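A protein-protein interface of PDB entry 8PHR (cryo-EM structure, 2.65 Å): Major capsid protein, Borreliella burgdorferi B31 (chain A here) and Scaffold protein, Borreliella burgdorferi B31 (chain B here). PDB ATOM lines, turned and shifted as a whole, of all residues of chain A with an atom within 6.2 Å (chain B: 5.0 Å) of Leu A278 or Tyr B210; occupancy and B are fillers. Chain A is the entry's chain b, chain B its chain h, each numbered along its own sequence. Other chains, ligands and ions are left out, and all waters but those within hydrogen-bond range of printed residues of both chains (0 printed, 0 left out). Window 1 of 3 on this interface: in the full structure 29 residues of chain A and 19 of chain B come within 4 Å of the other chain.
Of the printed residues of chain B, Lys A275 touches Ser B207.
Of the printed residues of chain B, Leu A278 touches Tyr B210.
Of the printed residues of chain A, Arg B213 touches Ile A17 and Val A20.
The nearest residue of chain A that does not touch Tyr B210 is Tyr A119 (4.7 Å).
Hydrophobic or aromatic side chains of chain B that line the printed part of chain A: Tyr B210.
Hydrophobic or aromatic side chains of chain A that line the printed part of chain B: Ile A17, Tyr A26, Tyr A276 and Leu A278.
Among the printed residues, 8 pairs touch across the chains.
Among the printed residues, no Asp or Glu carboxylate lies within 4 Å of a Lys or Arg side-chain nitrogen of the other chain.
Tyr B210 touches Ile A17.
NH1 of Arg B213 touches O of Ile A17, at 3.7 Å.
CE2 of Tyr A26 touches CB of Arg B214, at 3.5 Å.
Ser B207 touches Tyr A276 (OG to CE1, 3.2 Å).
Tyr B210 touches Leu A278 (CD1 to CD1, 3.4 Å).
Pro A279 touches Tyr B210 (O to CE2, 3.6 Å).
The guanidinium group (NH1) of Arg B213 sits at hydrogen-bond distance from the backbone carbonyl oxygen (O) of Val A20.
O of Lys A275 sits at hydrogen-bond distance from OG of Ser B207 (3.3 Å).
OG of Ser A274 sits at hydrogen-bond distance from N of Tyr A276.
O of Leu A278 lies within hydrogen-bond range of OG1 of Thr A280.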
ATOM      1  N   ILE A  17     -22.955  18.135  13.457  1.00  0.00           N
ATOM      2  CA  ILE A  17     -23.585  19.448  13.550  1.00  0.00           C
ATOM      3  C   ILE A  17     -24.245  19.837  12.232  1.00  0.00           C
ATOM      4  O   ILE A  17     -25.210  20.612  12.217  1.00  0.00           O
ATOM      5  CB  ILE A  17     -22.557  20.501  14.009  1.00  0.00           C
ATOM      6  CG1 ILE A  17     -23.263  21.776  14.473  1.00  0.00           C
ATOM      7  CG2 ILE A  17     -21.557  20.808  12.900  1.00  0.00           C
ATOM      8  CD1 ILE A  17     -24.196  21.558  15.646  1.00  0.00           C
ATOM      9  N   VAL A  20     -28.195  19.130  11.741  1.00  0.00           N
ATOM     10  CA  VAL A  20     -29.188  19.806  12.567  1.00  0.00           C
ATOM     11  C   VAL A  20     -29.873  20.876  11.727  1.00  0.00           C
ATOM     12  O   VAL A  20     -29.208  21.709  11.100  1.00  0.00           O
ATOM     13  CB  VAL A  20     -28.541  20.414  13.822  1.00  0.00           C
ATOM     14  CG1 VAL A  20     -29.603  21.015  14.725  1.00  0.00           C
ATOM     15  CG2 VAL A  20     -27.737  19.359  14.566  1.00  0.00           C
ATOM     16  N   PRO A  23     -33.222  26.844  12.608  1.00  0.00           N
ATOM     17  CA  PRO A  23     -34.441  27.249  13.317  1.00  0.00           C
ATOM     18  C   PRO A  23     -35.433  27.922  12.381  1.00  0.00           C
ATOM     19  O   PRO A  23     -35.058  28.571  11.401  1.00  0.00           O
ATOM     20  CB  PRO A  23     -33.926  28.226  14.383  1.00  0.00           C
ATOM     21  CG  PRO A  23     -32.458  27.941  14.497  1.00  0.00           C
ATOM     22  CD  PRO A  23     -32.028  27.530  13.127  1.00  0.00           C
ATOM     23  N   MET A  25     -37.383  30.336  13.277  1.00  0.00           N
ATOM     24  CA  MET A  25     -37.522  31.745  13.627  1.00  0.00           C
ATOM     25  C   MET A  25     -36.904  32.666  12.582  1.00  0.00           C
ATOM     26  O   MET A  25     -37.239  33.855  12.548  1.00  0.00           O
ATOM     27  CB  MET A  25     -36.883  32.009  14.991  1.00  0.00           C
ATOM     28  CG  MET A  25     -35.379  31.797  15.013  1.00  0.00           C
ATOM     29  SD  MET A  25     -34.659  31.984  16.654  1.00  0.00           S
ATOM     30  CE  MET A  25     -32.949  31.575  16.316  1.00  0.00           C
ATOM     31  N   TYR A  26     -36.011  32.145  11.736  1.00  0.00           N
ATOM     32  CA  TYR A  26     -35.375  32.973  10.718  1.00  0.00           C
ATOM     33  C   TYR A  26     -36.386  33.498   9.706  1.00  0.00           C
ATOM     34  O   TYR A  26     -36.206  34.593   9.161  1.00  0.00           O
ATOM     35  CB  TYR A  26     -34.281  32.177  10.006  1.00  0.00           C
ATOM     36  CG  TYR A  26     -33.039  31.935  10.834  1.00  0.00           C
ATOM     37  CD1 TYR A  26     -32.932  32.430  12.128  1.00  0.00           C
ATOM     38  CD2 TYR A  26     -31.977  31.203  10.323  1.00  0.00           C
ATOM     39  CE1 TYR A  26     -31.798  32.206  12.886  1.00  0.00           C
ATOM     40  CE2 TYR A  26     -30.841  30.973  11.074  1.00  0.00           C
ATOM     41  CZ  TYR A  26     -30.756  31.477  12.353  1.00  0.00           C
ATOM     42  OH  TYR A  26     -29.626  31.251  13.104  1.00  0.00           O
ATOM     43  N   TYR A 119     -26.786  13.906  21.210  1.00  0.00           N
ATOM     44  CA  TYR A 119     -26.518  15.328  21.034  1.00  0.00           C
ATOM     45  C   TYR A 119     -27.425  15.934  19.974  1.00  0.00           C
ATOM     46  O   TYR A 119     -27.919  17.052  20.140  1.00  0.00           O
ATOM     47  CB  TYR A 119     -25.050  15.543  20.669  1.00  0.00           C
ATOM     48  CG  TYR A 119     -24.723  16.965  20.275  1.00  0.00           C
ATOM     49  CD1 TYR A 119     -24.797  17.996  21.201  1.00  0.00           C
ATOM     50  CD2 TYR A 119     -24.346  17.277  18.976  1.00  0.00           C
ATOM     51  CE1 TYR A 119     -24.503  19.298  20.846  1.00  0.00           C
ATOM     52  CE2 TYR A 119     -24.049  18.576  18.611  1.00  0.00           C
ATOM     53  CZ  TYR A 119     -24.129  19.582  19.550  1.00  0.00           C
ATOM     54  OH  TYR A 119     -23.835  20.878  19.192  1.00  0.00           O
ATOM     55  N   SER A 123     -30.050  18.840  20.803  1.00  0.00           N
ATOM     56  CA  SER A 123     -29.953  20.110  20.095  1.00  0.00           C
ATOM     57  C   SER A 123     -31.265  20.460  19.409  1.00  0.00           C
ATOM     58  O   SER A 123     -31.683  21.621  19.415  1.00  0.00           O
ATOM     59  CB  SER A 123     -28.812  20.057  19.077  1.00  0.00           C
ATOM     60  OG  SER A 123     -27.572  19.805  19.714  1.00  0.00           O
ATOM     61  N   ILE A 126     -33.637  21.666  22.079  1.00  0.00           N
ATOM     62  CA  ILE A 126     -33.245  22.983  22.567  1.00  0.00           C
ATOM     63  C   ILE A 126     -33.596  24.060  21.549  1.00  0.00           C
ATOM     64  O   ILE A 126     -34.037  25.153  21.915  1.00  0.00           O
ATOM     65  CB  ILE A 126     -31.748  22.999  22.924  1.00  0.00           C
ATOM     66  CG1 ILE A 126     -31.492  22.122  24.148  1.00  0.00           C
ATOM     67  CG2 ILE A 126     -31.283  24.416  23.214  1.00  0.00           C
ATOM     68  CD1 ILE A 126     -30.040  22.039  24.542  1.00  0.00           C
ATOM     69  N   ILE A 127     -33.406  23.776  20.258  1.00  0.00           N
ATOM     70  CA  ILE A 127     -33.769  24.745  19.227  1.00  0.00           C
ATOM     71  C   ILE A 127     -35.278  24.958  19.196  1.00  0.00           C
ATOM     72  O   ILE A 127     -35.753  26.083  18.988  1.00  0.00           O
ATOM     73  CB  ILE A 127     -33.221  24.303  17.858  1.00  0.00           C
ATOM     74  CG1 ILE A 127     -31.692  24.333  17.866  1.00  0.00           C
ATOM     75  CG2 ILE A 127     -33.760  25.190  16.745  1.00  0.00           C
ATOM     76  CD1 ILE A 127     -31.066  23.707  16.648  1.00  0.00           C
ATOM     77  N   ILE A 130     -35.938  27.279  22.000  1.00  0.00           N
ATOM     78  CA  ILE A 130     -35.474  28.628  21.682  1.00  0.00           C
ATOM     79  C   ILE A 130     -36.459  29.329  20.756  1.00  0.00           C
ATOM     80  O   ILE A 130     -36.760  30.513  20.934  1.00  0.00           O
ATOM     81  CB  ILE A 130     -34.057  28.581  21.078  1.00  0.00           C
ATOM     82  CG1 ILE A 130     -33.051  28.085  22.118  1.00  0.00           C
ATOM     83  CG2 ILE A 130     -33.649  29.951  20.557  1.00  0.00           C
ATOM     84  CD1 ILE A 130     -31.645  27.935  21.584  1.00  0.00           C
ATOM     85  N   SER A 274     -27.162  36.805  20.997  1.00  0.00           N
ATOM     86  CA  SER A 274     -25.772  36.464  21.245  1.00  0.00           C
ATOM     87  C   SER A 274     -25.242  35.555  20.144  1.00  0.00           C
ATOM     88  O   SER A 274     -25.997  34.845  19.474  1.00  0.00           O
ATOM     89  CB  SER A 274     -25.625  35.778  22.601  1.00  0.00           C
ATOM     90  OG  SER A 274     -24.406  35.059  22.679  1.00  0.00           O
ATOM     91  N   LYS A 275     -23.925  35.583  19.959  1.00  0.00           N
ATOM     92  CA  LYS A 275     -23.278  34.689  19.010  1.00  0.00           C
ATOM     93  C   LYS A 275     -23.177  33.261  19.528  1.00  0.00           C
ATOM     94  O   LYS A 275     -22.682  32.389  18.806  1.00  0.00           O
ATOM     95  CB  LYS A 275     -21.884  35.217  18.658  1.00  0.00           C
ATOM     96  CG  LYS A 275     -20.989  35.458  19.860  1.00  0.00           C
ATOM     97  CD  LYS A 275     -19.584  35.842  19.428  1.00  0.00           C
ATOM     98  CE  LYS A 275     -18.973  34.782  18.529  1.00  0.00           C
ATOM     99  NZ  LYS A 275     -17.570  35.111  18.161  1.00  0.00           N
ATOM    100  N   TYR A 276     -23.635  33.005  20.754  1.00  0.00           N
ATOM    101  CA  TYR A 276     -23.654  31.671  21.339  1.00  0.00           C
ATOM    102  C   TYR A 276     -25.072  31.275  21.741  1.00  0.00           C
ATOM    103  O   TYR A 276     -25.265  30.418  22.606  1.00  0.00           O
ATOM    104  CB  TYR A 276     -22.719  31.597  22.544  1.00  0.00           C
ATOM    105  CG  TYR A 276     -21.326  32.117  22.274  1.00  0.00           C
ATOM    106  CD1 TYR A 276     -20.494  31.494  21.353  1.00  0.00           C
ATOM    107  CD2 TYR A 276     -20.842  33.233  22.943  1.00  0.00           C
ATOM    108  CE1 TYR A 276     -19.220  31.971  21.105  1.00  0.00           C
ATOM    109  CE2 TYR A 276     -19.571  33.716  22.703  1.00  0.00           C
ATOM    110  CZ  TYR A 276     -18.764  33.081  21.784  1.00  0.00           C
ATOM    111  OH  TYR A 276     -17.496  33.560  21.541  1.00  0.00           O
ATOM    112  N   MET A 277     -26.074  31.902  21.119  1.00  0.00           N
ATOM    113  CA  MET A 277     -27.462  31.617  21.466  1.00  0.00           C
ATOM    114  C   MET A 277     -27.838  30.182  21.117  1.00  0.00           C
ATOM    115  O   MET A 277     -28.510  29.501  21.900  1.00  0.00           O
ATOM    116  CB  MET A 277     -28.393  32.600  20.755  1.00  0.00           C
ATOM    117  CG  MET A 277     -29.784  32.051  20.476  1.00  0.00           C
ATOM    118  SD  MET A 277     -30.809  33.178  19.512  1.00  0.00           S
ATOM    119  CE  MET A 277     -29.992  33.093  17.921  1.00  0.00           C
ATOM    120  N   LEU A 278     -27.409  29.709  19.952  1.00  0.00           N
ATOM    121  CA  LEU A 278     -27.717  28.358  19.527  1.00  0.00           C
ATOM    122  C   LEU A 278     -26.916  27.354  20.356  1.00  0.00           C
ATOM    123  O   LEU A 278     -25.895  27.705  20.952  1.00  0.00           O
ATOM    124  CB  LEU A 278     -27.428  28.206  18.035  1.00  0.00           C
ATOM    125  CG  LEU A 278     -28.383  29.028  17.162  1.00  0.00           C
ATOM    126  CD1 LEU A 278     -28.253  28.663  15.694  1.00  0.00           C
ATOM    127  CD2 LEU A 278     -29.824  28.863  17.629  1.00  0.00           C
ATOM    128  N   PRO A 279     -27.375  26.100  20.426  1.00  0.00           N
ATOM    129  CA  PRO A 279     -26.731  25.127  21.319  1.00  0.00           C
ATOM    130  C   PRO A 279     -25.248  24.954  21.023  1.00  0.00           C
ATOM    131  O   PRO A 279     -24.824  24.911  19.866  1.00  0.00           O
ATOM    132  CB  PRO A 279     -27.508  23.836  21.043  1.00  0.00           C
ATOM    133  CG  PRO A 279     -28.850  24.302  20.620  1.00  0.00           C
ATOM    134  CD  PRO A 279     -28.613  25.561  19.834  1.00  0.00           C
ATOM    135  N   THR A 280     -24.458  24.852  22.096  1.00  0.00           N
ATOM    136  CA  THR A 280     -23.019  24.647  21.996  1.00  0.00           C
ATOM    137  C   THR A 280     -22.614  23.604  23.032  1.00  0.00           C
ATOM    138  O   THR A 280     -22.988  23.728  24.211  1.00  0.00           O
ATOM    139  CB  THR A 280     -22.244  25.950  22.215  1.00  0.00           C
ATOM    140  OG1 THR A 280     -22.765  26.971  21.356  1.00  0.00           O
ATOM    141  CG2 THR A 280     -20.765  25.752  21.914  1.00  0.00           C
ATOM    142  N   ASP A 298     -24.964  24.269  26.236  1.00  0.00           N
ATOM    143  CA  ASP A 298     -25.229  25.633  26.670  1.00  0.00           C
ATOM    144  C   ASP A 298     -25.921  26.421  25.565  1.00  0.00           C
ATOM    145  O   ASP A 298     -25.679  26.199  24.375  1.00  0.00           O
ATOM    146  CB  ASP A 298     -23.932  26.345  27.068  1.00  0.00           C
ATOM    147  CG  ASP A 298     -23.478  25.992  28.469  1.00  0.00           C
ATOM    148  OD1 ASP A 298     -24.206  26.319  29.429  1.00  0.00           O
ATOM    149  OD2 ASP A 298     -22.392  25.392  28.613  1.00  0.00           O
ATOM    150  N   PHE A 299     -26.791  27.344  25.973  1.00  0.00           N
ATOM    151  CA  PHE A 299     -27.474  28.222  25.033  1.00  0.00           C
ATOM    152  C   PHE A 299     -27.842  29.527  25.725  1.00  0.00           C
ATOM    153  O   PHE A 299     -28.090  29.560  26.933  1.00  0.00           O
ATOM    154  CB  PHE A 299     -28.720  27.552  24.435  1.00  0.00           C
ATOM    155  CG  PHE A 299     -29.794  27.245  25.440  1.00  0.00           C
ATOM    156  CD1 PHE A 299     -29.699  26.130  26.257  1.00  0.00           C
ATOM    157  CD2 PHE A 299     -30.908  28.060  25.556  1.00  0.00           C
ATOM    158  CE1 PHE A 299     -30.688  25.841  27.176  1.00  0.00           C
ATOM    159  CE2 PHE A 299     -31.900  27.776  26.474  1.00  0.00           C
ATOM    160  CZ  PHE A 299     -31.790  26.664  27.284  1.00  0.00           C
ATOM    161  N   VAL A 300     -27.894  30.603  24.942  1.00  0.00           N
ATOM    162  CA  VAL A 300     -28.090  31.952  25.460  1.00  0.00           C
ATOM    163  C   VAL A 300     -29.411  32.495  24.928  1.00  0.00           C
ATOM    164  O   VAL A 300     -29.701  32.377  23.732  1.00  0.00           O
ATOM    165  CB  VAL A 300     -26.922  32.880  25.077  1.00  0.00           C
ATOM    166  CG1 VAL A 300     -27.240  34.321  25.448  1.00  0.00           C
ATOM    167  CG2 VAL A 300     -25.637  32.419  25.748  1.00  0.00           C
ATOM    168  N   ALA B 205     -15.467  28.214  15.893  1.00  0.00           N
ATOM    169  CA  ALA B 205     -15.802  27.633  14.599  1.00  0.00           C
ATOM    170  C   ALA B 205     -17.274  27.253  14.529  1.00  0.00           C
ATOM    171  O   ALA B 205     -17.915  27.421  13.486  1.00  0.00           O
ATOM    172  CB  ALA B 205     -14.920  26.417  14.325  1.00  0.00           C
ATOM    173  N   ILE B 206     -17.827  26.731  15.627  1.00  0.00           N
ATOM    174  CA  ILE B 206     -19.253  26.411  15.658  1.00  0.00           C
ATOM    175  C   ILE B 206     -20.089  27.670  15.457  1.00  0.00           C
ATOM    176  O   ILE B 206     -21.066  27.672  14.697  1.00  0.00           O
ATOM    177  CB  ILE B 206     -19.617  25.696  16.974  1.00  0.00           C
ATOM    178  CG1 ILE B 206     -18.954  24.322  17.044  1.00  0.00           C
ATOM    179  CG2 ILE B 206     -21.126  25.561  17.112  1.00  0.00           C
ATOM    180  CD1 ILE B 206     -19.181  23.613  18.359  1.00  0.00           C
ATOM    181  N   SER B 207     -19.722  28.756  16.143  1.00  0.00           N
ATOM    182  CA  SER B 207     -20.464  30.006  15.996  1.00  0.00           C
ATOM    183  C   SER B 207     -20.373  30.540  14.569  1.00  0.00           C
ATOM    184  O   SER B 207     -21.378  30.986  13.995  1.00  0.00           O
ATOM    185  CB  SER B 207     -19.946  31.043  16.992  1.00  0.00           C
ATOM    186  OG  SER B 207     -19.951  30.527  18.312  1.00  0.00           O
ATOM    187  N   ASN B 208     -19.175  30.501  13.980  1.00  0.00           N
ATOM    188  CA  ASN B 208     -19.013  30.957  12.602  1.00  0.00           C
ATOM    189  C   ASN B 208     -19.817  30.094  11.638  1.00  0.00           C
ATOM    190  O   ASN B 208     -20.409  30.606  10.683  1.00  0.00           O
ATOM    191  CB  ASN B 208     -17.533  30.959  12.219  1.00  0.00           C
ATOM    192  CG  ASN B 208     -16.700  31.849  13.116  1.00  0.00           C
ATOM    193  OD1 ASN B 208     -17.228  32.537  13.990  1.00  0.00           O
ATOM    194  ND2 ASN B 208     -15.389  31.841  12.907  1.00  0.00           N
ATOM    195  N   THR B 209     -19.842  28.779  11.870  1.00  0.00           N
ATOM    196  CA  THR B 209     -20.626  27.888  11.025  1.00  0.00           C
ATOM    197  C   THR B 209     -22.113  28.197  11.131  1.00  0.00           C
ATOM    198  O   THR B 209     -22.828  28.189  10.124  1.00  0.00           O
ATOM    199  CB  THR B 209     -20.350  26.431  11.402  1.00  0.00           C
ATOM    200  OG1 THR B 209     -18.953  26.153  11.241  1.00  0.00           O
ATOM    201  CG2 THR B 209     -21.152  25.487  10.519  1.00  0.00           C
ATOM    202  N   TYR B 210     -22.599  28.468  12.345  1.00  0.00           N
ATOM    203  CA  TYR B 210     -24.002  28.838  12.509  1.00  0.00           C
ATOM    204  C   TYR B 210     -24.318  30.132  11.767  1.00  0.00           C
ATOM    205  O   TYR B 210     -25.361  30.244  11.105  1.00  0.00           O
ATOM    206  CB  TYR B 210     -24.341  28.979  13.992  1.00  0.00           C
ATOM    207  CG  TYR B 210     -24.767  27.691  14.658  1.00  0.00           C
ATOM    208  CD1 TYR B 210     -25.767  26.899  14.110  1.00  0.00           C
ATOM    209  CD2 TYR B 210     -24.183  27.277  15.848  1.00  0.00           C
ATOM    210  CE1 TYR B 210     -26.166  25.725  14.721  1.00  0.00           C
ATOM    211  CE2 TYR B 210     -24.575  26.105  16.467  1.00  0.00           C
ATOM    212  CZ  TYR B 210     -25.565  25.333  15.899  1.00  0.00           C
ATOM    213  OH  TYR B 210     -25.957  24.166  16.512  1.00  0.00           O
ATOM    214  N   LYS B 211     -23.426  31.122  11.865  1.00  0.00           N
ATOM    215  CA  LYS B 211     -23.640  32.378  11.151  1.00  0.00           C
ATOM    216  C   LYS B 211     -23.658  32.160   9.641  1.00  0.00           C
ATOM    217  O   LYS B 211     -24.495  32.733   8.932  1.00  0.00           O
ATOM    218  CB  LYS B 211     -22.562  33.391  11.536  1.00  0.00           C
ATOM    219  CG  LYS B 211     -22.659  34.711  10.791  1.00  0.00           C
ATOM    220  CD  LYS B 211     -21.455  35.593  11.070  1.00  0.00           C
ATOM    221  CE  LYS B 211     -21.527  36.888  10.278  1.00  0.00           C
ATOM    222  NZ  LYS B 211     -20.315  37.727  10.480  1.00  0.00           N
ATOM    223  N   GLN B 212     -22.741  31.334   9.133  1.00  0.00           N
ATOM    224  CA  GLN B 212     -22.712  31.045   7.703  1.00  0.00           C
ATOM    225  C   GLN B 212     -23.966  30.301   7.260  1.00  0.00           C
ATOM    226  O   GLN B 212     -24.475  30.537   6.160  1.00  0.00           O
ATOM    227  CB  GLN B 212     -21.458  30.246   7.350  1.00  0.00           C
ATOM    228  CG  GLN B 212     -20.161  31.010   7.552  1.00  0.00           C
ATOM    229  CD  GLN B 212     -18.938  30.181   7.214  1.00  0.00           C
ATOM    230  OE1 GLN B 212     -19.048  29.011   6.851  1.00  0.00           O
ATOM    231  NE2 GLN B 212     -17.762  30.786   7.333  1.00  0.00           N
ATOM    232  N   ARG B 213     -24.471  29.390   8.096  1.00  0.00           N
ATOM    233  CA  ARG B 213     -25.717  28.703   7.772  1.00  0.00           C
ATOM    234  C   ARG B 213     -26.883  29.681   7.705  1.00  0.00           C
ATOM    235  O   ARG B 213     -27.734  29.581   6.814  1.00  0.00           O
ATOM    236  CB  ARG B 213     -25.997  27.600   8.793  1.00  0.00           C
ATOM    237  CG  ARG B 213     -25.018  26.439   8.743  1.00  0.00           C
ATOM    238  CD  ARG B 213     -25.703  25.121   9.062  1.00  0.00           C
ATOM    239  NE  ARG B 213     -26.512  25.205  10.272  1.00  0.00           N
ATOM    240  CZ  ARG B 213     -27.210  24.197  10.777  1.00  0.00           C
ATOM    241  NH1 ARG B 213     -27.218  23.005  10.204  1.00  0.00           N
ATOM    242  NH2 ARG B 213     -27.917  24.390  11.888  1.00  0.00           N
ATOM    243  N   ARG B 214     -26.940  30.633   8.640  1.00  0.00           N
ATOM    244  CA  ARG B 214     -27.991  31.647   8.585  1.00  0.00           C
ATOM    245  C   ARG B 214     -27.879  32.490   7.319  1.00  0.00           C
ATOM    246  O   ARG B 214     -28.887  32.784   6.661  1.00  0.00           O
ATOM    247  CB  ARG B 214     -27.932  32.537   9.827  1.00  0.00           C
ATOM    248  CG  ARG B 214     -28.891  33.717   9.784  1.00  0.00           C
ATOM    249  CD  ARG B 214     -28.385  34.875  10.626  1.00  0.00           C
ATOM    250  NE  ARG B 214     -27.957  34.438  11.949  1.00  0.00           N
ATOM    251  CZ  ARG B 214     -27.292  35.197  12.810  1.00  0.00           C
ATOM    252  NH1 ARG B 214     -26.957  36.444  12.518  1.00  0.00           N
ATOM    253  NH2 ARG B 214     -26.955  34.692  13.993  1.00  0.00           N
